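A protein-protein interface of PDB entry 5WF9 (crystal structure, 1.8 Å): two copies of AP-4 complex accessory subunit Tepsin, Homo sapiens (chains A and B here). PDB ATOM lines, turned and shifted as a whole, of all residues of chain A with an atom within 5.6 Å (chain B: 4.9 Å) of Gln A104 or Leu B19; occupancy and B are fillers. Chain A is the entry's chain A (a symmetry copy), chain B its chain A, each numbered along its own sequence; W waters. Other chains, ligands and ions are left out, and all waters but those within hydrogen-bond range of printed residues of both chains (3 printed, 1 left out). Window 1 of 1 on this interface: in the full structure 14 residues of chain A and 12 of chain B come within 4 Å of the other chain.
The side-chain amide oxygen (OE1) of Gln A104 sits at hydrogen-bond distance from the guanidinium group (NH1) of Arg B15 (3.2 Å). The side-chain amide nitrogen (NE2) of Gln A130 sits at hydrogen-bond distance from the backbone carbonyl oxygen (O) of Leu B19 (3.0 Å). The side-chain amide nitrogen of Gln A104 is in hydrogen-bond range of the backbone carbonyl oxygen of Cys B57.
The guanidinium group of Arg B15 lies within hydrogen-bond range of the side-chain sulfur of Cys B57 (3.7 Å). The side-chain carboxylate of Glu B60 lies within salt-bridge range of the guanidinium group of Arg B15, 3.0 Å away. The side-chain hydroxyl of Ser A134 sits at hydrogen-bond distance from the backbone carbonyl oxygen of Gln A130 (3.0 Å).
Among the printed residues, merely in contact across the chains: Ala A101 with Arg B15 (3.5 Å), Ala A101 with Glu B60 (3.95 Å), Ile A103 with Leu B19 (3.9 Å), Gln A104 with Phe B18 (3.4 Å), Gln A104 with Leu B19 (3.7 Å), Gln A104 with Leu B22 (3.6 Å), Gln A104 with Glu B60 (3.8 Å), Gln A104 with Tyr B61 (3.8 Å), Ala A107 with Leu B19 (3.8 Å), Ala A107 with Leu B22 (3.3 Å), Ala A108 with Tyr B61 (3.8 Å), Gly A133 with Leu B16 (3.7 Å), Gly A133 with Leu B19 (3.6 Å), Ser A134 with Leu B16 (3.8 Å), Phe A137 with Arg B15 (3.7 Å) and Phe A137 with Leu B16 (3.7 Å).
Of the printed residues of chain B, Ala A101 touches Arg B15 (3.5 Å) and Glu B60 (3.95 Å). Of chain B, only Arg B15 (3.2 Å), Phe B18 (3.4 Å), Leu B19 (3.7 Å), Leu B22 (3.6 Å), Cys B57 (3.1 Å), Glu B60 (3.8 Å) and Tyr B61 (3.8 Å) come within 4 Å of Gln A104. Of the printed residues of chain B, Gly A133 touches Leu B16 (3.7 Å) and Leu B19 (3.6 Å). Printed residues of chain A within 4 Å of Arg B15: Ala A101, Gln A104 and Phe A137. Leu B19 touches five residues of chain A. His B20 touches none of the printed residues of chain A. Of the printed residues of chain A, Glu B60 touches Ala A101 and Gln A104. The nearest printed residue of chain B that does not touch Ser A134 is His B20 (4.4 Å).
Of the 12 printed residues of chain B, 8 touch a printed residue of chain A. Among the printed residues, 19 pairs touch across the chains. Among the printed residues, no Asp or Glu carboxylate lies within 4 Å of a Lys or Arg side-chain nitrogen of the other chain.
No position is printed for both chains. Of the 19 pairs that touch across the chains among the printed residues, none has its exchanged pair printed and touching as well.
Water W1 lies within hydrogen-bond range of the side-chain hydroxyl of Ser A134 (2.6 Å), the side-chain amide oxygen of Gln A130 (2.7 Å) and a ring nitrogen (NE2) of His B20 (3.4 Å). Water W3 lies within hydrogen-bond range of the side-chain amide oxygen (OE1) of Gln A104 and the backbone carbonyl oxygen (O) of Arg B15. Water W2 bridges the backbone carbonyl oxygen of Ala A101 (2.8 Å) and the side-chain carboxylate of Glu B60 (2.9 Å).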
ATOM      1  N   SER A 100       8.208  11.839  -8.299  1.00  0.00           N
ATOM      2  CA  SER A 100       8.854  12.989  -8.914  1.00  0.00           C
ATOM      3  C   SER A 100       9.262  12.750 -10.364  1.00  0.00           C
ATOM      4  O   SER A 100       9.957  13.586 -10.946  1.00  0.00           O
ATOM      5  CB  SER A 100      10.075  13.403  -8.088  1.00  0.00           C
ATOM      6  OG  SER A 100      10.957  12.313  -7.891  1.00  0.00           O
ATOM      7  N   ALA A 101       8.834  11.646 -10.973  1.00  0.00           N
ATOM      8  CA  ALA A 101       9.174  11.429 -12.371  1.00  0.00           C
ATOM      9  C   ALA A 101       8.554  12.483 -13.285  1.00  0.00           C
ATOM     10  O   ALA A 101       9.028  12.663 -14.410  1.00  0.00           O
ATOM     11  CB  ALA A 101       8.732  10.030 -12.800  1.00  0.00           C
ATOM     12  N   PHE A 102       7.513  13.187 -12.827  1.00  0.00           N
ATOM     13  CA  PHE A 102       6.864  14.184 -13.668  1.00  0.00           C
ATOM     14  C   PHE A 102       7.751  15.391 -13.928  1.00  0.00           C
ATOM     15  O   PHE A 102       7.497  16.136 -14.880  1.00  0.00           O
ATOM     16  CB  PHE A 102       5.561  14.650 -13.024  1.00  0.00           C
ATOM     17  CG  PHE A 102       5.766  15.491 -11.795  1.00  0.00           C
ATOM     18  CD1 PHE A 102       5.878  16.864 -11.887  1.00  0.00           C
ATOM     19  CD2 PHE A 102       5.872  14.898 -10.547  1.00  0.00           C
ATOM     20  CE1 PHE A 102       6.083  17.634 -10.767  1.00  0.00           C
ATOM     21  CE2 PHE A 102       6.071  15.663  -9.421  1.00  0.00           C
ATOM     22  CZ  PHE A 102       6.179  17.034  -9.530  1.00  0.00           C
ATOM     23  N   ILE A 103       8.778  15.611 -13.106  1.00  0.00           N
ATOM     24  CA  ILE A 103       9.525  16.855 -13.207  1.00  0.00           C
ATOM     25  C   ILE A 103      10.240  16.941 -14.546  1.00  0.00           C
ATOM     26  O   ILE A 103      10.208  17.984 -15.207  1.00  0.00           O
ATOM     27  CB  ILE A 103      10.492  17.003 -12.020  1.00  0.00           C
ATOM     28  CG1 ILE A 103       9.680  17.101 -10.724  1.00  0.00           C
ATOM     29  CG2 ILE A 103      11.376  18.243 -12.218  1.00  0.00           C
ATOM     30  CD1 ILE A 103      10.504  17.293  -9.453  1.00  0.00           C
ATOM     31  N   GLN A 104      10.877  15.853 -14.986  1.00  0.00           N
ATOM     32  CA  GLN A 104      11.565  15.924 -16.266  1.00  0.00           C
ATOM     33  C   GLN A 104      10.581  16.054 -17.418  1.00  0.00           C
ATOM     34  O   GLN A 104      10.958  16.556 -18.480  1.00  0.00           O
ATOM     35  CB  GLN A 104      12.483  14.713 -16.467  1.00  0.00           C
ATOM     36  CG  GLN A 104      11.797  13.378 -16.525  1.00  0.00           C
ATOM     37  CD  GLN A 104      12.788  12.237 -16.714  1.00  0.00           C
ATOM     38  OE1 GLN A 104      13.689  12.037 -15.895  1.00  0.00           O
ATOM     39  NE2 GLN A 104      12.629  11.494 -17.800  1.00  0.00           N
ATOM     40  N   GLU A 105       9.326  15.649 -17.225  1.00  0.00           N
ATOM     41  CA  GLU A 105       8.323  15.872 -18.259  1.00  0.00           C
ATOM     42  C   GLU A 105       7.905  17.334 -18.306  1.00  0.00           C
ATOM     43  O   GLU A 105       7.776  17.912 -19.391  1.00  0.00           O
ATOM     44  CB  GLU A 105       7.115  14.969 -18.018  1.00  0.00           C
ATOM     45  CG  GLU A 105       7.359  13.538 -18.463  1.00  0.00           C
ATOM     46  CD  GLU A 105       7.562  13.455 -19.963  1.00  0.00           C
ATOM     47  OE1 GLU A 105       6.573  13.644 -20.703  1.00  0.00           O
ATOM     48  OE2 GLU A 105       8.713  13.247 -20.406  1.00  0.00           O
ATOM     49  N   ALA A 106       7.694  17.947 -17.141  1.00  0.00           N
ATOM     50  CA  ALA A 106       7.421  19.379 -17.109  1.00  0.00           C
ATOM     51  C   ALA A 106       8.587  20.163 -17.687  1.00  0.00           C
ATOM     52  O   ALA A 106       8.392  21.168 -18.383  1.00  0.00           O
ATOM     53  CB  ALA A 106       7.129  19.824 -15.675  1.00  0.00           C
ATOM     54  N   ALA A 107       9.811  19.709 -17.425  1.00  0.00           N
ATOM     55  CA  ALA A 107      10.998  20.365 -17.942  1.00  0.00           C
ATOM     56  C   ALA A 107      11.179  20.163 -19.436  1.00  0.00           C
ATOM     57  O   ALA A 107      12.113  20.733 -20.006  1.00  0.00           O
ATOM     58  CB  ALA A 107      12.231  19.852 -17.194  1.00  0.00           C
ATOM     59  N   ALA A 108      10.319  19.373 -20.079  1.00  0.00           N
ATOM     60  CA  ALA A 108      10.360  19.186 -21.523  1.00  0.00           C
ATOM     61  C   ALA A 108       9.203  19.870 -22.238  1.00  0.00           C
ATOM     62  O   ALA A 108       9.041  19.697 -23.453  1.00  0.00           O
ATOM     63  CB  ALA A 108      10.376  17.695 -21.857  1.00  0.00           C
ATOM     64  N   ALA A 129      10.276  24.059 -13.676  1.00  0.00           N
ATOM     65  CA  ALA A 129      10.522  22.643 -13.423  1.00  0.00           C
ATOM     66  C   ALA A 129      11.975  22.398 -13.041  1.00  0.00           C
ATOM     67  O   ALA A 129      12.265  21.566 -12.169  1.00  0.00           O
ATOM     68  CB  ALA A 129      10.148  21.809 -14.651  1.00  0.00           C
ATOM     69  N   GLN A 130      12.905  23.087 -13.701  1.00  0.00           N
ATOM     70  CA  GLN A 130      14.314  22.954 -13.348  1.00  0.00           C
ATOM     71  C   GLN A 130      14.570  23.437 -11.925  1.00  0.00           C
ATOM     72  O   GLN A 130      15.302  22.794 -11.164  1.00  0.00           O
ATOM     73  CB  GLN A 130      15.173  23.732 -14.342  1.00  0.00           C
ATOM     74  CG  GLN A 130      15.205  23.135 -15.756  1.00  0.00           C
ATOM     75  CD  GLN A 130      16.128  21.935 -15.867  1.00  0.00           C
ATOM     76  OE1 GLN A 130      16.914  21.652 -14.961  1.00  0.00           O
ATOM     77  NE2 GLN A 130      16.033  21.220 -16.980  1.00  0.00           N
ATOM     78  N   GLY A 133      13.207  20.834  -9.521  1.00  0.00           N
ATOM     79  CA  GLY A 133      14.107  19.703  -9.440  1.00  0.00           C
ATOM     80  C   GLY A 133      15.365  20.016  -8.652  1.00  0.00           C
ATOM     81  O   GLY A 133      15.809  19.209  -7.834  1.00  0.00           O
ATOM     82  N   SER A 134      15.958  21.190  -8.889  1.00  0.00           N
ATOM     83  CA  SER A 134      17.153  21.570  -8.139  1.00  0.00           C
ATOM     84  C   SER A 134      16.862  21.631  -6.647  1.00  0.00           C
ATOM     85  O   SER A 134      17.692  21.228  -5.823  1.00  0.00           O
ATOM     86  CB  SER A 134      17.681  22.921  -8.627  1.00  0.00           C
ATOM     87  OG  SER A 134      18.083  22.849  -9.983  1.00  0.00           O
ATOM     88  N   PHE A 137      15.645  17.808  -5.354  1.00  0.00           N
ATOM     89  CA  PHE A 137      16.563  16.692  -5.556  1.00  0.00           C
ATOM     90  C   PHE A 137      17.929  16.896  -4.909  1.00  0.00           C
ATOM     91  O   PHE A 137      18.720  15.946  -4.863  1.00  0.00           O
ATOM     92  CB  PHE A 137      16.766  16.431  -7.060  1.00  0.00           C
ATOM     93  CG  PHE A 137      15.530  15.936  -7.781  1.00  0.00           C
ATOM     94  CD1 PHE A 137      14.563  15.193  -7.118  1.00  0.00           C
ATOM     95  CD2 PHE A 137      15.349  16.206  -9.127  1.00  0.00           C
ATOM     96  CE1 PHE A 137      13.438  14.732  -7.791  1.00  0.00           C
ATOM     97  CE2 PHE A 137      14.228  15.748  -9.803  1.00  0.00           C
ATOM     98  CZ  PHE A 137      13.275  15.011  -9.134  1.00  0.00           C
ATOM     99  N   ARG B  15      18.005  11.649 -11.136  1.00  0.00           N
ATOM    100  CA  ARG B  15      16.971  12.498 -11.717  1.00  0.00           C
ATOM    101  C   ARG B  15      17.479  13.919 -11.920  1.00  0.00           C
ATOM    102  O   ARG B  15      17.168  14.558 -12.931  1.00  0.00           O
ATOM    103  CB  ARG B  15      15.726  12.484 -10.830  1.00  0.00           C
ATOM    104  CG  ARG B  15      15.012  11.136 -10.829  1.00  0.00           C
ATOM    105  CD  ARG B  15      13.543  11.283 -11.163  1.00  0.00           C
ATOM    106  NE  ARG B  15      12.857   9.996 -11.300  1.00  0.00           N
ATOM    107  CZ  ARG B  15      12.415   9.475 -12.442  1.00  0.00           C
ATOM    108  NH1 ARG B  15      12.582  10.103 -13.597  1.00  0.00           N
ATOM    109  NH2 ARG B  15      11.789   8.307 -12.425  1.00  0.00           N
ATOM    110  N   LEU B  16      18.284  14.425 -10.984  1.00  0.00           N
ATOM    111  CA  LEU B  16      18.774  15.797 -11.088  1.00  0.00           C
ATOM    112  C   LEU B  16      19.833  15.929 -12.174  1.00  0.00           C
ATOM    113  O   LEU B  16      19.807  16.877 -12.970  1.00  0.00           O
ATOM    114  CB  LEU B  16      19.326  16.257  -9.737  1.00  0.00           C
ATOM    115  CG  LEU B  16      19.850  17.694  -9.682  1.00  0.00           C
ATOM    116  CD1 LEU B  16      18.770  18.694 -10.074  1.00  0.00           C
ATOM    117  CD2 LEU B  16      20.391  18.007  -8.290  1.00  0.00           C
ATOM    118  N   SER B  17      20.792  14.999 -12.208  1.00  0.00           N
ATOM    119  CA  SER B  17      21.763  14.987 -13.293  1.00  0.00           C
ATOM    120  C   SER B  17      21.057  14.977 -14.638  1.00  0.00           C
ATOM    121  O   SER B  17      21.438  15.708 -15.561  1.00  0.00           O
ATOM    122  CB  SER B  17      22.676  13.764 -13.164  1.00  0.00           C
ATOM    123  OG  SER B  17      23.420  13.818 -11.961  1.00  0.00           O
ATOM    124  N   PHE B  18      20.016  14.156 -14.765  1.00  0.00           N
ATOM    125  CA  PHE B  18      19.316  14.052 -16.037  1.00  0.00           C
ATOM    126  C   PHE B  18      18.627  15.358 -16.400  1.00  0.00           C
ATOM    127  O   PHE B  18      18.627  15.759 -17.568  1.00  0.00           O
ATOM    128  CB  PHE B  18      18.303  12.912 -15.992  1.00  0.00           C
ATOM    129  CG  PHE B  18      17.643  12.660 -17.309  1.00  0.00           C
ATOM    130  CD1 PHE B  18      18.297  11.940 -18.292  1.00  0.00           C
ATOM    131  CD2 PHE B  18      16.378  13.151 -17.578  1.00  0.00           C
ATOM    132  CE1 PHE B  18      17.699  11.706 -19.507  1.00  0.00           C
ATOM    133  CE2 PHE B  18      15.781  12.920 -18.803  1.00  0.00           C
ATOM    134  CZ  PHE B  18      16.443  12.197 -19.763  1.00  0.00           C
ATOM    135  N   LEU B  19      18.013  16.031 -15.420  1.00  0.00           N
ATOM    136  CA  LEU B  19      17.436  17.344 -15.692  1.00  0.00           C
ATOM    137  C   LEU B  19      18.450  18.272 -16.336  1.00  0.00           C
ATOM    138  O   LEU B  19      18.110  19.052 -17.232  1.00  0.00           O
ATOM    139  CB  LEU B  19      16.914  17.982 -14.403  1.00  0.00           C
ATOM    140  CG  LEU B  19      15.539  17.582 -13.886  1.00  0.00           C
ATOM    141  CD1 LEU B  19      15.217  18.431 -12.652  1.00  0.00           C
ATOM    142  CD2 LEU B  19      14.443  17.750 -14.940  1.00  0.00           C
ATOM    143  N   HIS B  20      19.702  18.225 -15.876  1.00  0.00           N
ATOM    144  CA  HIS B  20      20.718  19.109 -16.428  1.00  0.00           C
ATOM    145  C   HIS B  20      21.073  18.746 -17.862  1.00  0.00           C
ATOM    146  O   HIS B  20      21.686  19.560 -18.562  1.00  0.00           O
ATOM    147  CB  HIS B  20      21.966  19.073 -15.550  1.00  0.00           C
ATOM    148  CG  HIS B  20      21.737  19.597 -14.168  1.00  0.00           C
ATOM    149  ND1 HIS B  20      22.605  19.355 -13.125  1.00  0.00           N
ATOM    150  CD2 HIS B  20      20.729  20.341 -13.654  1.00  0.00           C
ATOM    151  CE1 HIS B  20      22.146  19.936 -12.030  1.00  0.00           C
ATOM    152  NE2 HIS B  20      21.009  20.539 -12.323  1.00  0.00           N
ATOM    153  N   ARG B  21      20.696  17.554 -18.315  1.00  0.00           N
ATOM    154  CA  ARG B  21      20.953  17.131 -19.686  1.00  0.00           C
ATOM    155  C   ARG B  21      19.819  17.482 -20.634  1.00  0.00           C
ATOM    156  O   ARG B  21      19.974  17.311 -21.847  1.00  0.00           O
ATOM    157  CB  ARG B  21      21.175  15.618 -19.748  1.00  0.00           C
ATOM    158  CG  ARG B  21      22.152  15.068 -18.728  1.00  0.00           C
ATOM    159  CD  ARG B  21      23.572  15.520 -18.985  1.00  0.00           C
ATOM    160  NE  ARG B  21      24.502  14.856 -18.073  1.00  0.00           N
ATOM    161  CZ  ARG B  21      24.770  15.258 -16.831  1.00  0.00           C
ATOM    162  NH1 ARG B  21      24.189  16.339 -16.330  1.00  0.00           N
ATOM    163  NH2 ARG B  21      25.625  14.574 -16.083  1.00  0.00           N
ATOM    164  N   LEU B  22      18.687  17.965 -20.123  1.00  0.00           N
ATOM    165  CA  LEU B  22      17.515  18.107 -20.975  1.00  0.00           C
ATOM    166  C   LEU B  22      17.703  19.077 -22.135  1.00  0.00           C
ATOM    167  O   LEU B  22      17.085  18.843 -23.187  1.00  0.00           O
ATOM    168  CB  LEU B  22      16.298  18.516 -20.132  1.00  0.00           C
ATOM    169  CG  LEU B  22      15.512  17.352 -19.526  1.00  0.00           C
ATOM    170  CD1 LEU B  22      14.339  17.882 -18.729  1.00  0.00           C
ATOM    171  CD2 LEU B  22      15.007  16.364 -20.581  1.00  0.00           C
ATOM    172  N   PRO B  23      18.495  20.143 -22.038  1.00  0.00           N
ATOM    173  CA  PRO B  23      18.760  20.938 -23.249  1.00  0.00           C
ATOM    174  C   PRO B  23      19.196  20.081 -24.430  1.00  0.00           C
ATOM    175  O   PRO B  23      18.724  20.290 -25.556  1.00  0.00           O
ATOM    176  CB  PRO B  23      19.856  21.900 -22.789  1.00  0.00           C
ATOM    177  CG  PRO B  23      19.609  22.065 -21.328  1.00  0.00           C
ATOM    178  CD  PRO B  23      19.111  20.739 -20.839  1.00  0.00           C
ATOM    179  N   CYS B  57      15.976   7.243 -16.723  1.00  0.00           N
ATOM    180  CA  CYS B  57      15.384   8.541 -17.033  1.00  0.00           C
ATOM    181  C   CYS B  57      15.313   8.760 -18.534  1.00  0.00           C
ATOM    182  O   CYS B  57      14.314   9.277 -19.053  1.00  0.00           O
ATOM    183  CB  CYS B  57      16.198   9.664 -16.393  1.00  0.00           C
ATOM    184  SG  CYS B  57      16.133   9.720 -14.586  1.00  0.00           S
ATOM    185  N   GLU B  60      12.412   6.757 -20.078  1.00  0.00           N
ATOM    186  CA  GLU B  60      11.157   7.437 -19.764  1.00  0.00           C
ATOM    187  C   GLU B  60      10.947   8.619 -20.696  1.00  0.00           C
ATOM    188  O   GLU B  60       9.853   8.826 -21.244  1.00  0.00           O
ATOM    189  CB  GLU B  60      11.178   7.927 -18.314  1.00  0.00           C
ATOM    190  CG  GLU B  60      11.124   6.852 -17.235  1.00  0.00           C
ATOM    191  CD  GLU B  60      11.141   7.456 -15.831  1.00  0.00           C
ATOM    192  OE1 GLU B  60      11.046   8.699 -15.715  1.00  0.00           O
ATOM    193  OE2 GLU B  60      11.267   6.698 -14.848  1.00  0.00           O
ATOM    194  N   TYR B  61      11.999   9.417 -20.872  1.00  0.00           N
ATOM    195  CA  TYR B  61      11.902  10.620 -21.688  1.00  0.00           C
ATOM    196  C   TYR B  61      11.617  10.273 -23.141  1.00  0.00           C
ATOM    197  O   TYR B  61      10.715  10.843 -23.762  1.00  0.00           O
ATOM    198  CB  TYR B  61      13.191  11.433 -21.578  1.00  0.00           C
ATOM    199  CG  TYR B  61      13.203  12.618 -22.514  1.00  0.00           C
ATOM    200  CD1 TYR B  61      12.671  13.840 -22.130  1.00  0.00           C
ATOM    201  CD2 TYR B  61      13.723  12.504 -23.795  1.00  0.00           C
ATOM    202  CE1 TYR B  61      12.668  14.924 -22.999  1.00  0.00           C
ATOM    203  CE2 TYR B  61      13.717  13.573 -24.671  1.00  0.00           C
ATOM    204  CZ  TYR B  61      13.192  14.783 -24.266  1.00  0.00           C
ATOM    205  OH  TYR B  61      13.195  15.850 -25.140  1.00  0.00           O
HETATM  206  O   HOH W   1      17.860  21.846 -12.422  1.00  0.00           O
HETATM  207  O   HOH W   2       9.255  10.823 -16.477  1.00  0.00           O
HETATM  208  O   HOH W   3      14.442  13.543 -13.756  1.00  0.00           O
